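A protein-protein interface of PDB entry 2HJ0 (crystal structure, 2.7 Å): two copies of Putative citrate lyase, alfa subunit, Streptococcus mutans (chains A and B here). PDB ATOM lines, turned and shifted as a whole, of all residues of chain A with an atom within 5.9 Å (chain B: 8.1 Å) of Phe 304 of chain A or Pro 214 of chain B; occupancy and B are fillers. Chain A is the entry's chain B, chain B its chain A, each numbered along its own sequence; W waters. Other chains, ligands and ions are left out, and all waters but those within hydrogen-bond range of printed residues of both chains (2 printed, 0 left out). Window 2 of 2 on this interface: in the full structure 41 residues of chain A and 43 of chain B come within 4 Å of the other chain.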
ATOM      1  N   PHE A 274      17.996 -25.640 -26.297  1.00  0.00           N
ATOM      2  CA  PHE A 274      17.272 -26.489 -25.352  1.00  0.00           C
ATOM      3  C   PHE A 274      18.060 -27.786 -25.123  1.00  0.00           C
ATOM      4  O   PHE A 274      18.780 -28.253 -26.010  1.00  0.00           O
ATOM      5  CB  PHE A 274      15.881 -26.811 -25.912  1.00  0.00           C
ATOM      6  CG  PHE A 274      15.878 -27.910 -26.935  1.00  0.00           C
ATOM      7  CD1 PHE A 274      15.631 -29.225 -26.552  1.00  0.00           C
ATOM      8  CD2 PHE A 274      16.180 -27.649 -28.264  1.00  0.00           C
ATOM      9  CE1 PHE A 274      15.688 -30.271 -27.469  1.00  0.00           C
ATOM     10  CE2 PHE A 274      16.241 -28.698 -29.197  1.00  0.00           C
ATOM     11  CZ  PHE A 274      15.994 -30.016 -28.792  1.00  0.00           C
ATOM     12  N   SER A 275      17.917 -28.367 -23.937  1.00  0.00           N
ATOM     13  CA  SER A 275      18.629 -29.597 -23.602  1.00  0.00           C
ATOM     14  C   SER A 275      17.689 -30.790 -23.590  1.00  0.00           C
ATOM     15  O   SER A 275      16.484 -30.624 -23.479  1.00  0.00           O
ATOM     16  CB  SER A 275      19.305 -29.464 -22.238  1.00  0.00           C
ATOM     17  OG  SER A 275      18.357 -29.091 -21.262  1.00  0.00           O
ATOM     18  N   PHE A 276      18.245 -31.995 -23.689  1.00  0.00           N
ATOM     19  CA  PHE A 276      17.422 -33.191 -23.707  1.00  0.00           C
ATOM     20  C   PHE A 276      18.239 -34.475 -23.519  1.00  0.00           C
ATOM     21  O   PHE A 276      19.459 -34.517 -23.713  1.00  0.00           O
ATOM     22  CB  PHE A 276      16.680 -33.298 -25.040  1.00  0.00           C
ATOM     23  CG  PHE A 276      17.583 -33.568 -26.179  1.00  0.00           C
ATOM     24  CD1 PHE A 276      18.308 -32.540 -26.757  1.00  0.00           C
ATOM     25  CD2 PHE A 276      17.778 -34.862 -26.626  1.00  0.00           C
ATOM     26  CE1 PHE A 276      19.232 -32.797 -27.778  1.00  0.00           C
ATOM     27  CE2 PHE A 276      18.702 -35.145 -27.650  1.00  0.00           C
ATOM     28  CZ  PHE A 276      19.433 -34.107 -28.229  1.00  0.00           C
ATOM     29  N   ALA A 302      20.171 -27.447 -30.215  1.00  0.00           N
ATOM     30  CA  ALA A 302      20.180 -27.772 -28.794  1.00  0.00           C
ATOM     31  C   ALA A 302      21.553 -27.469 -28.197  1.00  0.00           C
ATOM     32  O   ALA A 302      22.574 -27.623 -28.871  1.00  0.00           O
ATOM     33  CB  ALA A 302      19.847 -29.238 -28.607  1.00  0.00           C
ATOM     34  N   ASN A 303      21.583 -27.034 -26.938  1.00  0.00           N
ATOM     35  CA  ASN A 303      22.851 -26.733 -26.272  1.00  0.00           C
ATOM     36  C   ASN A 303      23.621 -27.995 -25.874  1.00  0.00           C
ATOM     37  O   ASN A 303      24.841 -28.041 -26.010  1.00  0.00           O
ATOM     38  CB  ASN A 303      22.626 -25.867 -25.029  1.00  0.00           C
ATOM     39  CG  ASN A 303      21.674 -26.507 -24.035  1.00  0.00           C
ATOM     40  OD1 ASN A 303      21.442 -25.966 -22.947  1.00  0.00           O
ATOM     41  ND2 ASN A 303      21.109 -27.662 -24.402  1.00  0.00           N
ATOM     42  N   PHE A 304      22.924 -29.019 -25.379  1.00  0.00           N
ATOM     43  CA  PHE A 304      23.603 -30.251 -24.992  1.00  0.00           C
ATOM     44  C   PHE A 304      22.679 -31.443 -24.809  1.00  0.00           C
ATOM     45  O   PHE A 304      21.471 -31.299 -24.622  1.00  0.00           O
ATOM     46  CB  PHE A 304      24.418 -30.059 -23.699  1.00  0.00           C
ATOM     47  CG  PHE A 304      23.577 -29.937 -22.447  1.00  0.00           C
ATOM     48  CD1 PHE A 304      23.109 -28.700 -22.022  1.00  0.00           C
ATOM     49  CD2 PHE A 304      23.228 -31.065 -21.711  1.00  0.00           C
ATOM     50  CE1 PHE A 304      22.303 -28.579 -20.885  1.00  0.00           C
ATOM     51  CE2 PHE A 304      22.421 -30.956 -20.572  1.00  0.00           C
ATOM     52  CZ  PHE A 304      21.960 -29.707 -20.164  1.00  0.00           C
ATOM     53  N   ALA A 305      23.280 -32.626 -24.869  1.00  0.00           N
ATOM     54  CA  ALA A 305      22.577 -33.888 -24.698  1.00  0.00           C
ATOM     55  C   ALA A 305      23.239 -34.561 -23.496  1.00  0.00           C
ATOM     56  O   ALA A 305      24.436 -34.372 -23.259  1.00  0.00           O
ATOM     57  CB  ALA A 305      22.732 -34.752 -25.952  1.00  0.00           C
ATOM     58  N   LEU A 306      22.475 -35.364 -22.761  1.00  0.00           N
ATOM     59  CA  LEU A 306      22.991 -36.014 -21.570  1.00  0.00           C
ATOM     60  C   LEU A 306      22.776 -37.519 -21.513  1.00  0.00           C
ATOM     61  O   LEU A 306      22.329 -38.142 -22.471  1.00  0.00           O
ATOM     62  CB  LEU A 306      22.337 -35.366 -20.350  1.00  0.00           C
ATOM     63  CG  LEU A 306      22.792 -35.795 -18.955  1.00  0.00           C
ATOM     64  CD1 LEU A 306      24.291 -35.484 -18.793  1.00  0.00           C
ATOM     65  CD2 LEU A 306      21.962 -35.066 -17.898  1.00  0.00           C
ATOM     66  N   VAL A 322      23.704 -30.301 -31.918  1.00  0.00           N
ATOM     67  CA  VAL A 322      23.795 -30.214 -30.475  1.00  0.00           C
ATOM     68  C   VAL A 322      25.209 -29.728 -30.179  1.00  0.00           C
ATOM     69  O   VAL A 322      26.197 -30.333 -30.600  1.00  0.00           O
ATOM     70  CB  VAL A 322      23.487 -31.583 -29.791  1.00  0.00           C
ATOM     71  CG1 VAL A 322      24.456 -32.650 -30.249  1.00  0.00           C
ATOM     72  CG2 VAL A 322      23.528 -31.425 -28.288  1.00  0.00           C
ATOM     73  N   ASP A 323      25.294 -28.604 -29.477  1.00  0.00           N
ATOM     74  CA  ASP A 323      26.575 -27.990 -29.159  1.00  0.00           C
ATOM     75  C   ASP A 323      27.529 -28.816 -28.320  1.00  0.00           C
ATOM     76  O   ASP A 323      28.672 -29.015 -28.709  1.00  0.00           O
ATOM     77  CB  ASP A 323      26.352 -26.649 -28.476  1.00  0.00           C
ATOM     78  CG  ASP A 323      27.592 -25.809 -28.473  1.00  0.00           C
ATOM     79  OD1 ASP A 323      28.060 -25.459 -29.584  1.00  0.00           O
ATOM     80  OD2 ASP A 323      28.114 -25.504 -27.376  1.00  0.00           O
ATOM     81  N   LYS A 324      27.077 -29.277 -27.162  1.00  0.00           N
ATOM     82  CA  LYS A 324      27.927 -30.072 -26.286  1.00  0.00           C
ATOM     83  C   LYS A 324      27.206 -31.339 -25.900  1.00  0.00           C
ATOM     84  O   LYS A 324      26.021 -31.502 -26.171  1.00  0.00           O
ATOM     85  CB  LYS A 324      28.238 -29.309 -25.006  1.00  0.00           C
ATOM     86  CG  LYS A 324      28.927 -27.992 -25.197  1.00  0.00           C
ATOM     87  CD  LYS A 324      30.417 -28.191 -25.241  1.00  0.00           C
ATOM     88  CE  LYS A 324      31.127 -26.855 -25.229  1.00  0.00           C
ATOM     89  NZ  LYS A 324      30.714 -26.016 -24.060  1.00  0.00           N
ATOM     90  N   ILE A 325      27.928 -32.234 -25.248  1.00  0.00           N
ATOM     91  CA  ILE A 325      27.335 -33.473 -24.780  1.00  0.00           C
ATOM     92  C   ILE A 325      28.024 -33.941 -23.489  1.00  0.00           C
ATOM     93  O   ILE A 325      29.237 -34.141 -23.461  1.00  0.00           O
ATOM     94  CB  ILE A 325      27.396 -34.545 -25.880  1.00  0.00           C
ATOM     95  CG1 ILE A 325      27.227 -35.931 -25.290  1.00  0.00           C
ATOM     96  CG2 ILE A 325      28.693 -34.479 -26.601  1.00  0.00           C
ATOM     97  CD1 ILE A 325      27.370 -36.976 -26.355  1.00  0.00           C
ATOM     98  N   LEU A 326      27.241 -34.076 -22.420  1.00  0.00           N
ATOM     99  CA  LEU A 326      27.754 -34.510 -21.126  1.00  0.00           C
ATOM    100  C   LEU A 326      27.506 -36.007 -21.022  1.00  0.00           C
ATOM    101  O   LEU A 326      26.372 -36.472 -21.180  1.00  0.00           O
ATOM    102  CB  LEU A 326      27.047 -33.760 -19.994  1.00  0.00           C
ATOM    103  CG  LEU A 326      27.035 -32.230 -20.159  1.00  0.00           C
ATOM    104  CD1 LEU A 326      26.340 -31.604 -18.980  1.00  0.00           C
ATOM    105  CD2 LEU A 326      28.445 -31.685 -20.284  1.00  0.00           C
ATOM    106  N   VAL A 363      23.728 -31.753 -13.497  1.00  0.00           N
ATOM    107  CA  VAL A 363      23.408 -31.405 -14.875  1.00  0.00           C
ATOM    108  C   VAL A 363      21.936 -31.658 -15.216  1.00  0.00           C
ATOM    109  O   VAL A 363      21.308 -30.841 -15.892  1.00  0.00           O
ATOM    110  CB  VAL A 363      24.302 -32.160 -15.889  1.00  0.00           C
ATOM    111  CG1 VAL A 363      25.763 -31.802 -15.647  1.00  0.00           C
ATOM    112  CG2 VAL A 363      24.097 -33.663 -15.763  1.00  0.00           C
ATOM    113  N   GLN A 366      19.508 -29.050 -15.356  1.00  0.00           N
ATOM    114  CA  GLN A 366      19.477 -28.107 -16.458  1.00  0.00           C
ATOM    115  C   GLN A 366      18.861 -28.790 -17.654  1.00  0.00           C
ATOM    116  O   GLN A 366      18.905 -28.276 -18.762  1.00  0.00           O
ATOM    117  CB  GLN A 366      20.892 -27.635 -16.790  1.00  0.00           C
ATOM    118  CG  GLN A 366      21.599 -27.014 -15.597  1.00  0.00           C
ATOM    119  CD  GLN A 366      20.820 -25.845 -15.013  1.00  0.00           C
ATOM    120  OE1 GLN A 366      20.933 -25.539 -13.823  1.00  0.00           O
ATOM    121  NE2 GLN A 366      20.031 -25.180 -15.854  1.00  0.00           N
ATOM    122  N   LEU A 367      18.257 -29.943 -17.418  1.00  0.00           N
ATOM    123  CA  LEU A 367      17.649 -30.708 -18.494  1.00  0.00           C
ATOM    124  C   LEU A 367      16.216 -30.240 -18.783  1.00  0.00           C
ATOM    125  O   LEU A 367      15.398 -30.186 -17.873  1.00  0.00           O
ATOM    126  CB  LEU A 367      17.667 -32.182 -18.099  1.00  0.00           C
ATOM    127  CG  LEU A 367      17.323 -33.225 -19.148  1.00  0.00           C
ATOM    128  CD1 LEU A 367      18.251 -33.126 -20.338  1.00  0.00           C
ATOM    129  CD2 LEU A 367      17.426 -34.589 -18.504  1.00  0.00           C
ATOM    130  N   SER B 172      33.404 -18.872 -16.754  1.00  0.00           N
ATOM    131  CA  SER B 172      32.531 -19.675 -15.911  1.00  0.00           C
ATOM    132  C   SER B 172      31.074 -19.537 -16.348  1.00  0.00           C
ATOM    133  O   SER B 172      30.686 -18.496 -16.875  1.00  0.00           O
ATOM    134  CB  SER B 172      32.671 -19.211 -14.463  1.00  0.00           C
ATOM    135  OG  SER B 172      31.660 -19.772 -13.644  1.00  0.00           O
ATOM    136  N   ASP B 173      30.267 -20.578 -16.168  1.00  0.00           N
ATOM    137  CA  ASP B 173      28.856 -20.445 -16.518  1.00  0.00           C
ATOM    138  C   ASP B 173      28.153 -19.958 -15.263  1.00  0.00           C
ATOM    139  O   ASP B 173      28.801 -19.709 -14.250  1.00  0.00           O
ATOM    140  CB  ASP B 173      28.234 -21.767 -16.995  1.00  0.00           C
ATOM    141  CG  ASP B 173      28.558 -22.941 -16.091  1.00  0.00           C
ATOM    142  OD1 ASP B 173      28.553 -22.761 -14.846  1.00  0.00           O
ATOM    143  OD2 ASP B 173      28.799 -24.049 -16.642  1.00  0.00           O
ATOM    144  N   ALA B 174      26.836 -19.826 -15.327  1.00  0.00           N
ATOM    145  CA  ALA B 174      26.082 -19.344 -14.188  1.00  0.00           C
ATOM    146  C   ALA B 174      25.782 -20.459 -13.218  1.00  0.00           C
ATOM    147  O   ALA B 174      24.842 -20.379 -12.432  1.00  0.00           O
ATOM    148  CB  ALA B 174      24.794 -18.695 -14.646  1.00  0.00           C
ATOM    149  N   TYR B 175      26.580 -21.509 -13.260  1.00  0.00           N
ATOM    150  CA  TYR B 175      26.359 -22.604 -12.336  1.00  0.00           C
ATOM    151  C   TYR B 175      27.651 -23.013 -11.650  1.00  0.00           C
ATOM    152  O   TYR B 175      27.623 -23.840 -10.739  1.00  0.00           O
ATOM    153  CB  TYR B 175      25.743 -23.794 -13.069  1.00  0.00           C
ATOM    154  CG  TYR B 175      24.664 -24.494 -12.275  1.00  0.00           C
ATOM    155  CD1 TYR B 175      23.615 -23.774 -11.698  1.00  0.00           C
ATOM    156  CD2 TYR B 175      24.657 -25.876 -12.142  1.00  0.00           C
ATOM    157  CE1 TYR B 175      22.585 -24.411 -11.022  1.00  0.00           C
ATOM    158  CE2 TYR B 175      23.626 -26.522 -11.460  1.00  0.00           C
ATOM    159  CZ  TYR B 175      22.591 -25.778 -10.908  1.00  0.00           C
ATOM    160  OH  TYR B 175      21.547 -26.416 -10.274  1.00  0.00           O
ATOM    161  N   ASN B 177      30.857 -24.091 -13.418  1.00  0.00           N
ATOM    162  CA  ASN B 177      31.898 -24.748 -14.210  1.00  0.00           C
ATOM    163  C   ASN B 177      32.842 -23.642 -14.715  1.00  0.00           C
ATOM    164  O   ASN B 177      32.432 -22.768 -15.484  1.00  0.00           O
ATOM    165  CB  ASN B 177      31.287 -25.496 -15.395  1.00  0.00           C
ATOM    166  CG  ASN B 177      30.371 -26.629 -14.966  1.00  0.00           C
ATOM    167  OD1 ASN B 177      30.802 -27.590 -14.318  1.00  0.00           O
ATOM    168  ND2 ASN B 177      29.094 -26.524 -15.331  1.00  0.00           N
ATOM    169  N   ALA B 178      34.101 -23.681 -14.284  1.00  0.00           N
ATOM    170  CA  ALA B 178      35.076 -22.661 -14.659  1.00  0.00           C
ATOM    171  C   ALA B 178      36.404 -23.226 -15.155  1.00  0.00           C
ATOM    172  O   ALA B 178      36.755 -24.374 -14.872  1.00  0.00           O
ATOM    173  CB  ALA B 178      35.330 -21.753 -13.460  1.00  0.00           C
ATOM    174  N   ASN B 179      37.148 -22.424 -15.904  1.00  0.00           N
ATOM    175  CA  ASN B 179      38.450 -22.877 -16.374  1.00  0.00           C
ATOM    176  C   ASN B 179      39.343 -21.662 -16.531  1.00  0.00           C
ATOM    177  O   ASN B 179      38.864 -20.532 -16.463  1.00  0.00           O
ATOM    178  CB  ASN B 179      38.335 -23.689 -17.687  1.00  0.00           C
ATOM    179  CG  ASN B 179      37.907 -22.855 -18.881  1.00  0.00           C
ATOM    180  OD1 ASN B 179      38.580 -21.904 -19.259  1.00  0.00           O
ATOM    181  ND2 ASN B 179      36.786 -23.228 -19.493  1.00  0.00           N
ATOM    182  N   VAL B 211      30.008 -17.423 -19.535  1.00  0.00           N
ATOM    183  CA  VAL B 211      29.765 -18.283 -20.673  1.00  0.00           C
ATOM    184  C   VAL B 211      28.471 -19.086 -20.520  1.00  0.00           C
ATOM    185  O   VAL B 211      28.075 -19.432 -19.406  1.00  0.00           O
ATOM    186  CB  VAL B 211      30.967 -19.232 -20.836  1.00  0.00           C
ATOM    187  CG1 VAL B 211      30.667 -20.326 -21.855  1.00  0.00           C
ATOM    188  CG2 VAL B 211      32.175 -18.417 -21.255  1.00  0.00           C
ATOM    189  N   PRO B 212      27.774 -19.363 -21.639  1.00  0.00           N
ATOM    190  CA  PRO B 212      26.532 -20.142 -21.542  1.00  0.00           C
ATOM    191  C   PRO B 212      26.823 -21.571 -21.071  1.00  0.00           C
ATOM    192  O   PRO B 212      27.874 -22.147 -21.375  1.00  0.00           O
ATOM    193  CB  PRO B 212      25.966 -20.085 -22.965  1.00  0.00           C
ATOM    194  CG  PRO B 212      27.199 -19.889 -23.821  1.00  0.00           C
ATOM    195  CD  PRO B 212      28.022 -18.916 -23.025  1.00  0.00           C
ATOM    196  N   TYR B 213      25.881 -22.125 -20.319  1.00  0.00           N
ATOM    197  CA  TYR B 213      25.999 -23.467 -19.774  1.00  0.00           C
ATOM    198  C   TYR B 213      25.864 -24.530 -20.856  1.00  0.00           C
ATOM    199  O   TYR B 213      25.026 -24.410 -21.748  1.00  0.00           O
ATOM    200  CB  TYR B 213      24.905 -23.678 -18.718  1.00  0.00           C
ATOM    201  CG  TYR B 213      25.015 -24.963 -17.930  1.00  0.00           C
ATOM    202  CD1 TYR B 213      24.607 -26.185 -18.475  1.00  0.00           C
ATOM    203  CD2 TYR B 213      25.544 -24.963 -16.644  1.00  0.00           C
ATOM    204  CE1 TYR B 213      24.726 -27.375 -17.754  1.00  0.00           C
ATOM    205  CE2 TYR B 213      25.669 -26.146 -15.918  1.00  0.00           C
ATOM    206  CZ  TYR B 213      25.260 -27.344 -16.480  1.00  0.00           C
ATOM    207  OH  TYR B 213      25.414 -28.511 -15.766  1.00  0.00           O
ATOM    208  N   PRO B 214      26.687 -25.583 -20.794  1.00  0.00           N
ATOM    209  CA  PRO B 214      27.727 -25.845 -19.791  1.00  0.00           C
ATOM    210  C   PRO B 214      29.082 -25.369 -20.315  1.00  0.00           C
ATOM    211  O   PRO B 214      29.374 -25.528 -21.497  1.00  0.00           O
ATOM    212  CB  PRO B 214      27.691 -27.356 -19.652  1.00  0.00           C
ATOM    213  CG  PRO B 214      27.434 -27.773 -21.084  1.00  0.00           C
ATOM    214  CD  PRO B 214      26.322 -26.831 -21.491  1.00  0.00           C
ATOM    215  N   ASN B 215      29.903 -24.794 -19.446  1.00  0.00           N
ATOM    216  CA  ASN B 215      31.215 -24.321 -19.853  1.00  0.00           C
ATOM    217  C   ASN B 215      32.191 -25.498 -19.852  1.00  0.00           C
ATOM    218  O   ASN B 215      32.092 -26.403 -19.011  1.00  0.00           O
ATOM    219  CB  ASN B 215      31.689 -23.224 -18.888  1.00  0.00           C
ATOM    220  CG  ASN B 215      33.078 -22.693 -19.224  1.00  0.00           C
ATOM    221  OD1 ASN B 215      33.491 -22.716 -20.382  1.00  0.00           O
ATOM    222  ND2 ASN B 215      33.799 -22.192 -18.206  1.00  0.00           N
ATOM    223  N   THR B 216      33.113 -25.494 -20.811  1.00  0.00           N
ATOM    224  CA  THR B 216      34.132 -26.537 -20.926  1.00  0.00           C
ATOM    225  C   THR B 216      35.359 -25.973 -21.646  1.00  0.00           C
ATOM    226  O   THR B 216      35.233 -25.079 -22.476  1.00  0.00           O
ATOM    227  CB  THR B 216      33.617 -27.769 -21.713  1.00  0.00           C
ATOM    228  OG1 THR B 216      33.001 -27.347 -22.932  1.00  0.00           O
ATOM    229  CG2 THR B 216      32.620 -28.567 -20.890  1.00  0.00           C
ATOM    230  N   PRO B 217      36.566 -26.465 -21.320  1.00  0.00           N
ATOM    231  CA  PRO B 217      36.895 -27.504 -20.337  1.00  0.00           C
ATOM    232  C   PRO B 217      36.443 -27.081 -18.942  1.00  0.00           C
ATOM    233  O   PRO B 217      36.059 -25.928 -18.734  1.00  0.00           O
ATOM    234  CB  PRO B 217      38.419 -27.590 -20.401  1.00  0.00           C
ATOM    235  CG  PRO B 217      38.771 -26.992 -21.699  1.00  0.00           C
ATOM    236  CD  PRO B 217      37.787 -25.883 -21.885  1.00  0.00           C
ATOM    237  N   ILE B 218      36.526 -28.002 -17.988  1.00  0.00           N
ATOM    238  CA  ILE B 218      36.116 -27.725 -16.618  1.00  0.00           C
ATOM    239  C   ILE B 218      37.241 -27.969 -15.619  1.00  0.00           C
ATOM    240  O   ILE B 218      37.595 -29.107 -15.352  1.00  0.00           O
ATOM    241  CB  ILE B 218      34.932 -28.598 -16.256  1.00  0.00           C
ATOM    242  CG1 ILE B 218      33.808 -28.366 -17.273  1.00  0.00           C
ATOM    243  CG2 ILE B 218      34.510 -28.310 -14.840  1.00  0.00           C
ATOM    244  CD1 ILE B 218      32.595 -29.286 -17.106  1.00  0.00           C
ATOM    245  N   GLN B 222      30.782 -27.398 -11.194  1.00  0.00           N
ATOM    246  CA  GLN B 222      29.663 -26.705 -10.565  1.00  0.00           C
ATOM    247  C   GLN B 222      29.409 -27.285  -9.167  1.00  0.00           C
ATOM    248  O   GLN B 222      28.908 -26.585  -8.282  1.00  0.00           O
ATOM    249  CB  GLN B 222      28.404 -26.847 -11.441  1.00  0.00           C
ATOM    250  CG  GLN B 222      28.033 -28.316 -11.735  1.00  0.00           C
ATOM    251  CD  GLN B 222      27.022 -28.496 -12.852  1.00  0.00           C
ATOM    252  OE1 GLN B 222      27.273 -28.100 -13.979  1.00  0.00           O
ATOM    253  NE2 GLN B 222      25.882 -29.111 -12.543  1.00  0.00           N
HETATM  254  O   HOH W   1      26.992 -25.458 -24.442  1.00  0.00           O
HETATM  255  O   HOH W   2      32.992 -24.110 -24.014  1.00  0.00           O
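O of Pro 214 of chain B sits at hydrogen-bond distance from NZ of Lys 324 of chain A, 2.9 Å away.
The side-chain amino group (NZ) of Lys 324 of chain A lies within hydrogen-bond range of the side-chain hydroxyl (OG1) of Thr 216 of chain B.
The backbone carbonyl oxygen of Asn 303 of chain A is in hydrogen-bond range of the backbone NH of Lys 324 of chain A, 2.8 Å away.
N of Ala 305 of chain A is in hydrogen-bond range of O of Lys 324 of chain A, 3.2 Å away.
O of Phe 304 of chain A sits at hydrogen-bond distance from N of Phe 276 of chain A, at 3.4 Å.
The side-chain hydroxyl (OG) of Ser 275 of chain A is in hydrogen-bond range of the backbone carbonyl oxygen (O) of Gln 366 of chain A, at 2.7 Å.
The backbone NH (N) of Tyr 175 of chain B sits at hydrogen-bond distance from the side-chain carboxylate (OD1) of Asp 173 of chain B, 2.8 Å away.
The side-chain amide oxygen (OE1) of Gln 222 of chain B is in hydrogen-bond range of the side-chain amide nitrogen (ND2) of Asn 177 of chain B, 2.8 Å away.
Among the printed residues, pairs that only touch across the chains: Phe 304 of chain A with Pro 214 of chain B, Val 363 of chain A with Tyr 213 of chain B, Val 363 of chain A with Gln 222 of chain B, Gln 366 of chain A with Tyr 175 of chain B and Gln 366 of chain A with Tyr 213 of chain B.
Phe 304 of chain A touches just one residue of chain B: Pro 214.
Pro 214 of chain B touches just these residues of chain A: Phe 304 (3.8 Å) and Lys 324 (2.9 Å).
No residue of chain B comes within 4 Å of Asn 303 of chain A.
Printed residues of chain B within 4 Å of Val 363 of chain A: Tyr 213 (3.3 Å) and Gln 222 (3.5 Å).
Printed residues of chain B within 4 Å of Lys 324 of chain A: Pro 214 and Thr 216.
Of the printed residues of chain A, Gln 222 of chain B touches Val 363 (3.5 Å).
Printed residues of chain A within 4 Å of Thr 216 of chain B: Lys 324.
The nearest residue of chain B that does not touch Phe 304 of chain A is Tyr 213 of chain B (4.1 Å).
The nearest residue of chain A that does not touch Pro 214 of chain B is Leu 326 of chain A (4.1 Å).
Printed residues of chain A that touch a printed residue of chain B: Phe 304, Lys 324, Val 363 and Gln 366.
Hydrophobic or aromatic side chains of chain A that line the printed part of chain B: Phe 304 and Val 363.
Among the printed residues, 7 pairs touch across the chains.
Among the printed residues, no Asp or Glu carboxylate lies within 4 Å of a Lys or Arg side-chain nitrogen of the other chain.
No position is printed for both chains.
Water W2 lies within hydrogen-bond range of O of Thr 216 of chain B (2.9 Å) and NZ of Lys 324 of chain A (3.0 Å).
Water W1 lies within hydrogen-bond range of the side-chain carboxylate of Asp 323 of chain A (3.1 Å) and the backbone carbonyl oxygen of Tyr 213 of chain B (3.5 Å).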
